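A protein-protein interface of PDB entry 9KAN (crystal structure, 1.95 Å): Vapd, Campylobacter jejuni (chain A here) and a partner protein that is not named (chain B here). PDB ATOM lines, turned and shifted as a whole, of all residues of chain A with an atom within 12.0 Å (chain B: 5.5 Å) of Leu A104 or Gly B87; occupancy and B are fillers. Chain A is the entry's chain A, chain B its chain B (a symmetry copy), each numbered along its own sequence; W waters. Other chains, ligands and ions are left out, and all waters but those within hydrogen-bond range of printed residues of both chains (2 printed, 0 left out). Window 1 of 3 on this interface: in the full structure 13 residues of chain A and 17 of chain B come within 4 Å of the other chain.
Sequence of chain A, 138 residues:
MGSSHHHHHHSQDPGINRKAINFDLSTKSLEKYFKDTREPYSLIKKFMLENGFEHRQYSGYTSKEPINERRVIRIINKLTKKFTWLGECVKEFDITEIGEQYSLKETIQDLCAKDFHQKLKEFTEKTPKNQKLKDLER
Of the 10 printed residues of chain B, 6 touch a printed residue of chain A.
Printed residues of chain B that touch a printed residue of chain A: Tyr B84, Asp B85, Leu B86, Gly B87, Thr B90 and Leu B91.
Along chain B the printed residues that touch a printed residue of chain A span positions 84 to 91.
Of the 17 printed residues of chain A, 5 touch a printed residue of chain B.
Hydrophobic or aromatic side chains of chain A within 4 Å of the printed part of chain B: Tyr A102 and Leu A104.
Of chain B, only Gly B87 (3.6 Å) comes within 4 Å of Leu A104.
Of chain A, only Leu A104 (3.6 Å) and Thr A107 (3.1 Å) come within 4 Å of Gly B87.
Leu B86 touches just one residue of chain A: Tyr A102.
No residue of chain A comes within 4 Å of Cys B88.
Thr B90 touches one residue of chain A.
Printed residues of chain A within 4 Å of Tyr B84: Ser A103.
Of the printed residues of chain B, Thr A107 touches Gly B87 (3.1 Å), Thr B90 (3.9 Å) and Leu B91 (3.9 Å).
Printed residues of chain B within 4 Å of Asp A110: Leu B91.
Of the printed residues of chain B, Tyr A102 touches Asp B85 and Leu B86.
Glu A106 touches none of the printed residues of chain B.
The nearest residue of chain B that does not touch Leu A104 is Leu B86 (4.2 Å).
O of Tyr B84 sits at hydrogen-bond distance from SG of Cys B88 (3.2 Å).
OG1 of Thr B90 lies within hydrogen-bond range of O of Leu B86, at 2.7 Å.
Asp B85 touches Tyr A102.
CD2 of Tyr A102 touches CD1 of Leu B86 (3.5 Å).
OG of Ser A103 touches CE1 of Tyr B84, at 3.96 Å.
CD2 of Leu A104 touches CA of Gly B87 (3.6 Å).
Thr A107 touches Gly B87.
CG2 of Thr A107 touches CB of Thr B90 (3.9 Å).
CD2 of Leu B91 touches CG2 of Thr A107, 3.9 Å away.
OD2 of Asp A110 touches CD1 of Leu B91, 3.5 Å away.
Water W1 lies within hydrogen-bond range of OH of Tyr A102 (2.5 Å) and OD2 of Asp B85 (2.6 Å).
Water W2 lies within hydrogen-bond range of N of Gly B87, O of Ser A103 and N of Leu B86.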
ATOM      1  N   ARG A  56     -28.170   0.966  23.705  1.00  0.00           N
ATOM      2  CA  ARG A  56     -27.196   1.437  22.692  1.00  0.00           C
ATOM      3  C   ARG A  56     -27.858   1.404  21.312  1.00  0.00           C
ATOM      4  O   ARG A  56     -28.835   0.642  21.139  1.00  0.00           O
ATOM      5  CB  ARG A  56     -25.961   0.532  22.707  1.00  0.00           C
ATOM      6  CG  ARG A  56     -25.264   0.448  24.057  1.00  0.00           C
ATOM      7  CD  ARG A  56     -25.167   1.806  24.731  1.00  0.00           C
ATOM      8  NE  ARG A  56     -23.971   2.545  24.318  1.00  0.00           N
ATOM      9  CZ  ARG A  56     -23.988   3.746  23.757  1.00  0.00           C
ATOM     10  NH1 ARG A  56     -24.793   3.988  22.738  1.00  0.00           N
ATOM     11  NH2 ARG A  56     -23.200   4.700  24.216  1.00  0.00           N
ATOM     12  N   GLN A  57     -27.328   2.181  20.366  1.00  0.00           N
ATOM     13  CA  GLN A  57     -27.863   2.175  18.981  1.00  0.00           C
ATOM     14  C   GLN A  57     -27.281   0.968  18.232  1.00  0.00           C
ATOM     15  O   GLN A  57     -27.418   0.917  16.991  1.00  0.00           O
ATOM     16  CB  GLN A  57     -27.493   3.487  18.290  1.00  0.00           C
ATOM     17  CG  GLN A  57     -25.992   3.729  18.180  1.00  0.00           C
ATOM     18  CD  GLN A  57     -25.403   4.448  19.374  1.00  0.00           C
ATOM     19  OE1 GLN A  57     -26.079   4.692  20.381  1.00  0.00           O
ATOM     20  NE2 GLN A  57     -24.128   4.792  19.278  1.00  0.00           N
ATOM     21  N   TYR A  58     -26.652   0.055  18.973  1.00  0.00           N
ATOM     22  CA  TYR A  58     -26.122  -1.191  18.360  1.00  0.00           C
ATOM     23  C   TYR A  58     -26.794  -2.347  19.092  1.00  0.00           C
ATOM     24  O   TYR A  58     -27.655  -3.008  18.468  1.00  0.00           O
ATOM     25  CB  TYR A  58     -24.590  -1.249  18.409  1.00  0.00           C
ATOM     26  CG  TYR A  58     -23.935  -1.280  19.785  1.00  0.00           C
ATOM     27  CD1 TYR A  58     -23.687  -2.480  20.444  1.00  0.00           C
ATOM     28  CD2 TYR A  58     -23.603  -0.103  20.442  1.00  0.00           C
ATOM     29  CE1 TYR A  58     -23.101  -2.508  21.697  1.00  0.00           C
ATOM     30  CE2 TYR A  58     -23.024  -0.117  21.700  1.00  0.00           C
ATOM     31  CZ  TYR A  58     -22.771  -1.322  22.329  1.00  0.00           C
ATOM     32  OH  TYR A  58     -22.198  -1.337  23.567  1.00  0.00           O
ATOM     33  N   GLU A 100     -12.897   2.124  28.958  1.00  0.00           N
ATOM     34  CA  GLU A 100     -12.889   3.374  28.209  1.00  0.00           C
ATOM     35  C   GLU A 100     -13.688   3.142  26.935  1.00  0.00           C
ATOM     36  O   GLU A 100     -13.644   2.034  26.396  1.00  0.00           O
ATOM     37  CB  GLU A 100     -11.470   3.787  27.840  1.00  0.00           C
ATOM     38  CG  GLU A 100     -11.269   5.238  27.917  1.00  0.00           C
ATOM     39  CD  GLU A 100     -11.245   5.683  29.347  1.00  0.00           C
ATOM     40  OE1 GLU A 100     -10.328   5.229  30.065  1.00  0.00           O
ATOM     41  OE2 GLU A 100     -12.156   6.448  29.749  1.00  0.00           O
ATOM     42  N   GLN A 101     -14.420   4.141  26.436  1.00  0.00           N
ATOM     43  CA  GLN A 101     -15.178   3.989  25.198  1.00  0.00           C
ATOM     44  C   GLN A 101     -14.837   5.124  24.241  1.00  0.00           C
ATOM     45  O   GLN A 101     -14.925   6.298  24.611  1.00  0.00           O
ATOM     46  CB  GLN A 101     -16.683   3.953  25.461  1.00  0.00           C
ATOM     47  CG  GLN A 101     -17.499   3.863  24.180  1.00  0.00           C
ATOM     48  CD  GLN A 101     -18.956   3.504  24.422  1.00  0.00           C
ATOM     49  OE1 GLN A 101     -19.269   2.442  24.961  1.00  0.00           O
ATOM     50  NE2 GLN A 101     -19.855   4.392  24.011  1.00  0.00           N
ATOM     51  N   TYR A 102     -14.451   4.769  23.011  1.00  0.00           N
ATOM     52  CA  TYR A 102     -13.926   5.714  22.031  1.00  0.00           C
ATOM     53  C   TYR A 102     -14.822   5.743  20.801  1.00  0.00           C
ATOM     54  O   TYR A 102     -15.322   4.701  20.367  1.00  0.00           O
ATOM     55  CB  TYR A 102     -12.496   5.336  21.606  1.00  0.00           C
ATOM     56  CG  TYR A 102     -11.457   5.497  22.692  1.00  0.00           C
ATOM     57  CD1 TYR A 102     -11.041   6.762  23.098  1.00  0.00           C
ATOM     58  CD2 TYR A 102     -10.888   4.385  23.319  1.00  0.00           C
ATOM     59  CE1 TYR A 102     -10.088   6.920  24.104  1.00  0.00           C
ATOM     60  CE2 TYR A 102      -9.931   4.538  24.329  1.00  0.00           C
ATOM     61  CZ  TYR A 102      -9.533   5.808  24.708  1.00  0.00           C
ATOM     62  OH  TYR A 102      -8.587   5.964  25.695  1.00  0.00           O
ATOM     63  N   SER A 103     -15.035   6.933  20.240  1.00  0.00           N
ATOM     64  CA  SER A 103     -15.910   7.097  19.086  1.00  0.00           C
ATOM     65  C   SER A 103     -15.086   7.264  17.811  1.00  0.00           C
ATOM     66  O   SER A 103     -14.227   8.145  17.730  1.00  0.00           O
ATOM     67  CB  SER A 103     -16.836   8.295  19.269  1.00  0.00           C
ATOM     68  OG  SER A 103     -17.508   8.579  18.055  1.00  0.00           O
ATOM     69  N   LEU A 104     -15.364   6.423  16.813  1.00  0.00           N
ATOM     70  CA  LEU A 104     -14.650   6.482  15.546  1.00  0.00           C
ATOM     71  C   LEU A 104     -15.517   6.887  14.356  1.00  0.00           C
ATOM     72  O   LEU A 104     -15.007   6.906  13.227  1.00  0.00           O
ATOM     73  CB  LEU A 104     -13.979   5.130  15.257  1.00  0.00           C
ATOM     74  CG  LEU A 104     -12.725   4.870  16.098  1.00  0.00           C
ATOM     75  CD1 LEU A 104     -12.095   3.552  15.725  1.00  0.00           C
ATOM     76  CD2 LEU A 104     -11.697   6.002  15.968  1.00  0.00           C
ATOM     77  N   LYS A 105     -16.792   7.243  14.566  1.00  0.00           N
ATOM     78  CA  LYS A 105     -17.670   7.585  13.445  1.00  0.00           C
ATOM     79  C   LYS A 105     -17.048   8.648  12.544  1.00  0.00           C
ATOM     80  O   LYS A 105     -16.848   8.429  11.344  1.00  0.00           O
ATOM     81  CB  LYS A 105     -19.032   8.068  13.950  1.00  0.00           C
ATOM     82  CG  LYS A 105     -19.897   8.666  12.826  1.00  0.00           C
ATOM     83  CD  LYS A 105     -21.200   9.274  13.325  1.00  0.00           C
ATOM     84  CE  LYS A 105     -20.970  10.543  14.154  1.00  0.00           C
ATOM     85  NZ  LYS A 105     -21.102  11.829  13.387  1.00  0.00           N
ATOM     86  N   GLU A 106     -16.738   9.813  13.113  1.00  0.00           N
ATOM     87  CA  GLU A 106     -16.175  10.897  12.320  1.00  0.00           C
ATOM     88  C   GLU A 106     -14.804  10.538  11.741  1.00  0.00           C
ATOM     89  O   GLU A 106     -14.476  10.964  10.628  1.00  0.00           O
ATOM     90  CB  GLU A 106     -16.094  12.160  13.179  1.00  0.00           C
ATOM     91  CG  GLU A 106     -15.136  13.221  12.666  1.00  0.00           C
ATOM     92  CD  GLU A 106     -15.708  14.032  11.513  1.00  0.00           C
ATOM     93  OE1 GLU A 106     -15.544  13.629  10.341  1.00  0.00           O
ATOM     94  OE2 GLU A 106     -16.323  15.086  11.776  1.00  0.00           O
ATOM     95  N   THR A 107     -13.990   9.767  12.472  1.00  0.00           N
ATOM     96  CA  THR A 107     -12.681   9.381  11.956  1.00  0.00           C
ATOM     97  C   THR A 107     -12.815   8.530  10.702  1.00  0.00           C
ATOM     98  O   THR A 107     -12.086   8.731   9.725  1.00  0.00           O
ATOM     99  CB  THR A 107     -11.897   8.618  13.017  1.00  0.00           C
ATOM    100  OG1 THR A 107     -11.988   9.311  14.266  1.00  0.00           O
ATOM    101  CG2 THR A 107     -10.425   8.517  12.613  1.00  0.00           C
ATOM    102  N   ILE A 108     -13.740   7.571  10.726  1.00  0.00           N
ATOM    103  CA  ILE A 108     -14.014   6.714   9.574  1.00  0.00           C
ATOM    104  C   ILE A 108     -14.516   7.545   8.394  1.00  0.00           C
ATOM    105  O   ILE A 108     -14.111   7.328   7.242  1.00  0.00           O
ATOM    106  CB  ILE A 108     -15.013   5.613   9.994  1.00  0.00           C
ATOM    107  CG1 ILE A 108     -14.293   4.548  10.843  1.00  0.00           C
ATOM    108  CG2 ILE A 108     -15.748   5.019   8.791  1.00  0.00           C
ATOM    109  CD1 ILE A 108     -15.213   3.582  11.552  1.00  0.00           C
ATOM    110  N   GLN A 109     -15.389   8.524   8.660  1.00  0.00           N
ATOM    111  CA  GLN A 109     -15.788   9.467   7.616  1.00  0.00           C
ATOM    112  C   GLN A 109     -14.583  10.249   7.076  1.00  0.00           C
ATOM    113  O   GLN A 109     -14.465  10.459   5.861  1.00  0.00           O
ATOM    114  CB  GLN A 109     -16.872  10.408   8.160  1.00  0.00           C
ATOM    115  CG  GLN A 109     -18.199   9.693   8.515  1.00  0.00           C
ATOM    116  CD  GLN A 109     -19.155  10.568   9.333  1.00  0.00           C
ATOM    117  OE1 GLN A 109     -18.740  11.569   9.915  1.00  0.00           O
ATOM    118  NE2 GLN A 109     -20.435  10.191   9.376  1.00  0.00           N
ATOM    119  N   ASP A 110     -13.664  10.660   7.962  1.00  0.00           N
ATOM    120  CA  ASP A 110     -12.464  11.383   7.536  1.00  0.00           C
ATOM    121  C   ASP A 110     -11.585  10.524   6.644  1.00  0.00           C
ATOM    122  O   ASP A 110     -11.088  10.996   5.617  1.00  0.00           O
ATOM    123  CB  ASP A 110     -11.650  11.848   8.746  1.00  0.00           C
ATOM    124  CG  ASP A 110     -12.117  13.184   9.290  1.00  0.00           C
ATOM    125  OD1 ASP A 110     -13.194  13.651   8.870  1.00  0.00           O
ATOM    126  OD2 ASP A 110     -11.398  13.769  10.135  1.00  0.00           O
ATOM    127  N   LEU A 111     -11.359   9.269   7.037  1.00  0.00           N
ATOM    128  CA  LEU A 111     -10.471   8.403   6.271  1.00  0.00           C
ATOM    129  C   LEU A 111     -10.967   8.232   4.840  1.00  0.00           C
ATOM    130  O   LEU A 111     -10.177   8.288   3.891  1.00  0.00           O
ATOM    131  CB  LEU A 111     -10.335   7.049   6.967  1.00  0.00           C
ATOM    132  CG  LEU A 111      -9.520   7.025   8.263  1.00  0.00           C
ATOM    133  CD1 LEU A 111      -9.784   5.733   9.035  1.00  0.00           C
ATOM    134  CD2 LEU A 111      -8.019   7.218   8.004  1.00  0.00           C
ATOM    135  N   CYS A 112     -12.276   8.093   4.674  1.00  0.00           N
ATOM    136  CA  CYS A 112     -12.855   7.888   3.324  1.00  0.00           C
ATOM    137  C   CYS A 112     -13.108   9.253   2.654  1.00  0.00           C
ATOM    138  O   CYS A 112     -14.160   9.390   2.016  1.00  0.00           O
ATOM    139  CB  CYS A 112     -14.146   7.082   3.436  1.00  0.00           C
ATOM    140  SG  CYS A 112     -14.059   5.622   4.502  1.00  0.00           S
ATOM    141  N   ALA A 113     -12.168  10.198   2.779  1.00  0.00           N
ATOM    142  CA  ALA A 113     -12.322  11.529   2.139  1.00  0.00           C
ATOM    143  C   ALA A 113     -11.333  11.685   0.980  1.00  0.00           C
ATOM    144  O   ALA A 113     -11.531  12.604   0.158  1.00  0.00           O
ATOM    145  CB  ALA A 113     -12.147  12.632   3.160  1.00  0.00           C
ATOM    146  N   SER B  67      -5.735  17.023  12.945  1.00  0.00           N
ATOM    147  CA  SER B  67      -6.076  15.773  13.614  1.00  0.00           C
ATOM    148  C   SER B  67      -6.642  15.966  15.016  1.00  0.00           C
ATOM    149  O   SER B  67      -7.118  14.988  15.605  1.00  0.00           O
ATOM    150  CB  SER B  67      -4.853  14.861  13.692  1.00  0.00           C
ATOM    151  OG  SER B  67      -4.292  14.680  12.408  1.00  0.00           O
ATOM    152  N   TYR B  84     -12.703  10.998  21.686  1.00  0.00           N
ATOM    153  CA  TYR B  84     -12.172  11.082  20.329  1.00  0.00           C
ATOM    154  C   TYR B  84     -10.663  10.856  20.251  1.00  0.00           C
ATOM    155  O   TYR B  84     -10.089  11.036  19.169  1.00  0.00           O
ATOM    156  CB  TYR B  84     -12.525  12.435  19.702  1.00  0.00           C
ATOM    157  CG  TYR B  84     -14.012  12.725  19.665  1.00  0.00           C
ATOM    158  CD1 TYR B  84     -14.872  11.972  18.872  1.00  0.00           C
ATOM    159  CD2 TYR B  84     -14.557  13.751  20.434  1.00  0.00           C
ATOM    160  CE1 TYR B  84     -16.241  12.245  18.838  1.00  0.00           C
ATOM    161  CE2 TYR B  84     -15.908  14.028  20.406  1.00  0.00           C
ATOM    162  CZ  TYR B  84     -16.749  13.278  19.617  1.00  0.00           C
ATOM    163  OH  TYR B  84     -18.090  13.571  19.609  1.00  0.00           O
ATOM    164  N   ASP B  85     -10.012  10.452  21.355  1.00  0.00           N
ATOM    165  CA  ASP B  85      -8.552  10.298  21.374  1.00  0.00           C
ATOM    166  C   ASP B  85      -8.061   9.345  20.283  1.00  0.00           C
ATOM    167  O   ASP B  85      -7.104   9.647  19.564  1.00  0.00           O
ATOM    168  CB  ASP B  85      -8.079   9.780  22.731  1.00  0.00           C
ATOM    169  CG  ASP B  85      -8.055  10.854  23.806  1.00  0.00           C
ATOM    170  OD1 ASP B  85      -8.479  12.000  23.547  1.00  0.00           O
ATOM    171  OD2 ASP B  85      -7.619  10.538  24.931  1.00  0.00           O
ATOM    172  N   LEU B  86      -8.681   8.174  20.176  1.00  0.00           N
ATOM    173  CA  LEU B  86      -8.206   7.170  19.218  1.00  0.00           C
ATOM    174  C   LEU B  86      -8.346   7.661  17.787  1.00  0.00           C
ATOM    175  O   LEU B  86      -7.497   7.371  16.938  1.00  0.00           O
ATOM    176  CB  LEU B  86      -8.973   5.858  19.374  1.00  0.00           C
ATOM    177  CG  LEU B  86      -8.630   4.861  20.466  1.00  0.00           C
ATOM    178  CD1 LEU B  86      -9.479   3.607  20.214  1.00  0.00           C
ATOM    179  CD2 LEU B  86      -7.143   4.535  20.458  1.00  0.00           C
ATOM    180  N   GLY B  87      -9.418   8.394  17.496  1.00  0.00           N
ATOM    181  CA  GLY B  87      -9.593   8.920  16.150  1.00  0.00           C
ATOM    182  C   GLY B  87      -8.554   9.969  15.808  1.00  0.00           C
ATOM    183  O   GLY B  87      -8.041  10.011  14.690  1.00  0.00           O
ATOM    184  N   CYS B  88      -8.230  10.833  16.771  1.00  0.00           N
ATOM    185  CA  CYS B  88      -7.179  11.824  16.552  1.00  0.00           C
ATOM    186  C   CYS B  88      -5.836  11.155  16.312  1.00  0.00           C
ATOM    187  O   CYS B  88      -5.079  11.561  15.417  1.00  0.00           O
ATOM    188  CB  CYS B  88      -7.097  12.783  17.753  1.00  0.00           C
ATOM    189  SG  CYS B  88      -8.628  13.701  18.040  1.00  0.00           S
ATOM    190  N   MET B  89      -5.525  10.117  17.085  1.00  0.00           N
ATOM    191  CA  MET B  89      -4.292   9.389  16.845  1.00  0.00           C
ATOM    192  C   MET B  89      -4.310   8.667  15.501  1.00  0.00           C
ATOM    193  O   MET B  89      -3.260   8.546  14.862  1.00  0.00           O
ATOM    194  CB  MET B  89      -4.037   8.401  17.977  1.00  0.00           C
ATOM    195  CG  MET B  89      -3.656   9.082  19.306  1.00  0.00           C
ATOM    196  SD  MET B  89      -1.943   9.633  19.365  1.00  0.00           S
ATOM    197  CE  MET B  89      -1.138   8.058  19.500  1.00  0.00           C
ATOM    198  N   THR B  90      -5.473   8.173  15.068  1.00  0.00           N
ATOM    199  CA  THR B  90      -5.562   7.504  13.766  1.00  0.00           C
ATOM    200  C   THR B  90      -5.195   8.465  12.636  1.00  0.00           C
ATOM    201  O   THR B  90      -4.474   8.100  11.703  1.00  0.00           O
ATOM    202  CB  THR B  90      -6.975   6.944  13.547  1.00  0.00           C
ATOM    203  OG1 THR B  90      -7.296   5.990  14.572  1.00  0.00           O
ATOM    204  CG2 THR B  90      -7.067   6.250  12.183  1.00  0.00           C
ATOM    205  N   LEU B  91      -5.659   9.713  12.726  1.00  0.00           N
ATOM    206  CA  LEU B  91      -5.424  10.668  11.648  1.00  0.00           C
ATOM    207  C   LEU B  91      -3.973  11.135  11.632  1.00  0.00           C
ATOM    208  O   LEU B  91      -3.311  11.116  10.582  1.00  0.00           O
ATOM    209  CB  LEU B  91      -6.370  11.860  11.797  1.00  0.00           C
ATOM    210  CG  LEU B  91      -7.879  11.628  11.779  1.00  0.00           C
ATOM    211  CD1 LEU B  91      -8.589  12.947  11.981  1.00  0.00           C
ATOM    212  CD2 LEU B  91      -8.285  11.005  10.442  1.00  0.00           C
ATOM    213  N   PHE B  92      -3.466  11.555  12.800  1.00  0.00           N
ATOM    214  CA  PHE B  92      -2.127  12.119  12.918  1.00  0.00           C
ATOM    215  C   PHE B  92      -1.059  11.118  12.497  1.00  0.00           C
ATOM    216  O   PHE B  92      -0.147  11.449  11.731  1.00  0.00           O
ATOM    217  CB  PHE B  92      -1.900  12.576  14.366  1.00  0.00           C
ATOM    218  CG  PHE B  92      -0.692  13.453  14.568  1.00  0.00           C
ATOM    219  CD1 PHE B  92      -0.386  14.479  13.677  1.00  0.00           C
ATOM    220  CD2 PHE B  92       0.104  13.298  15.699  1.00  0.00           C
ATOM    221  CE1 PHE B  92       0.707  15.309  13.896  1.00  0.00           C
ATOM    222  CE2 PHE B  92       1.191  14.135  15.924  1.00  0.00           C
ATOM    223  CZ  PHE B  92       1.489  15.145  15.013  1.00  0.00           C
HETATM  224  O   HOH W   1      -7.351   8.180  25.924  1.00  0.00           O
HETATM  225  O   HOH W   2     -11.682   7.923  19.348  1.00  0.00           O
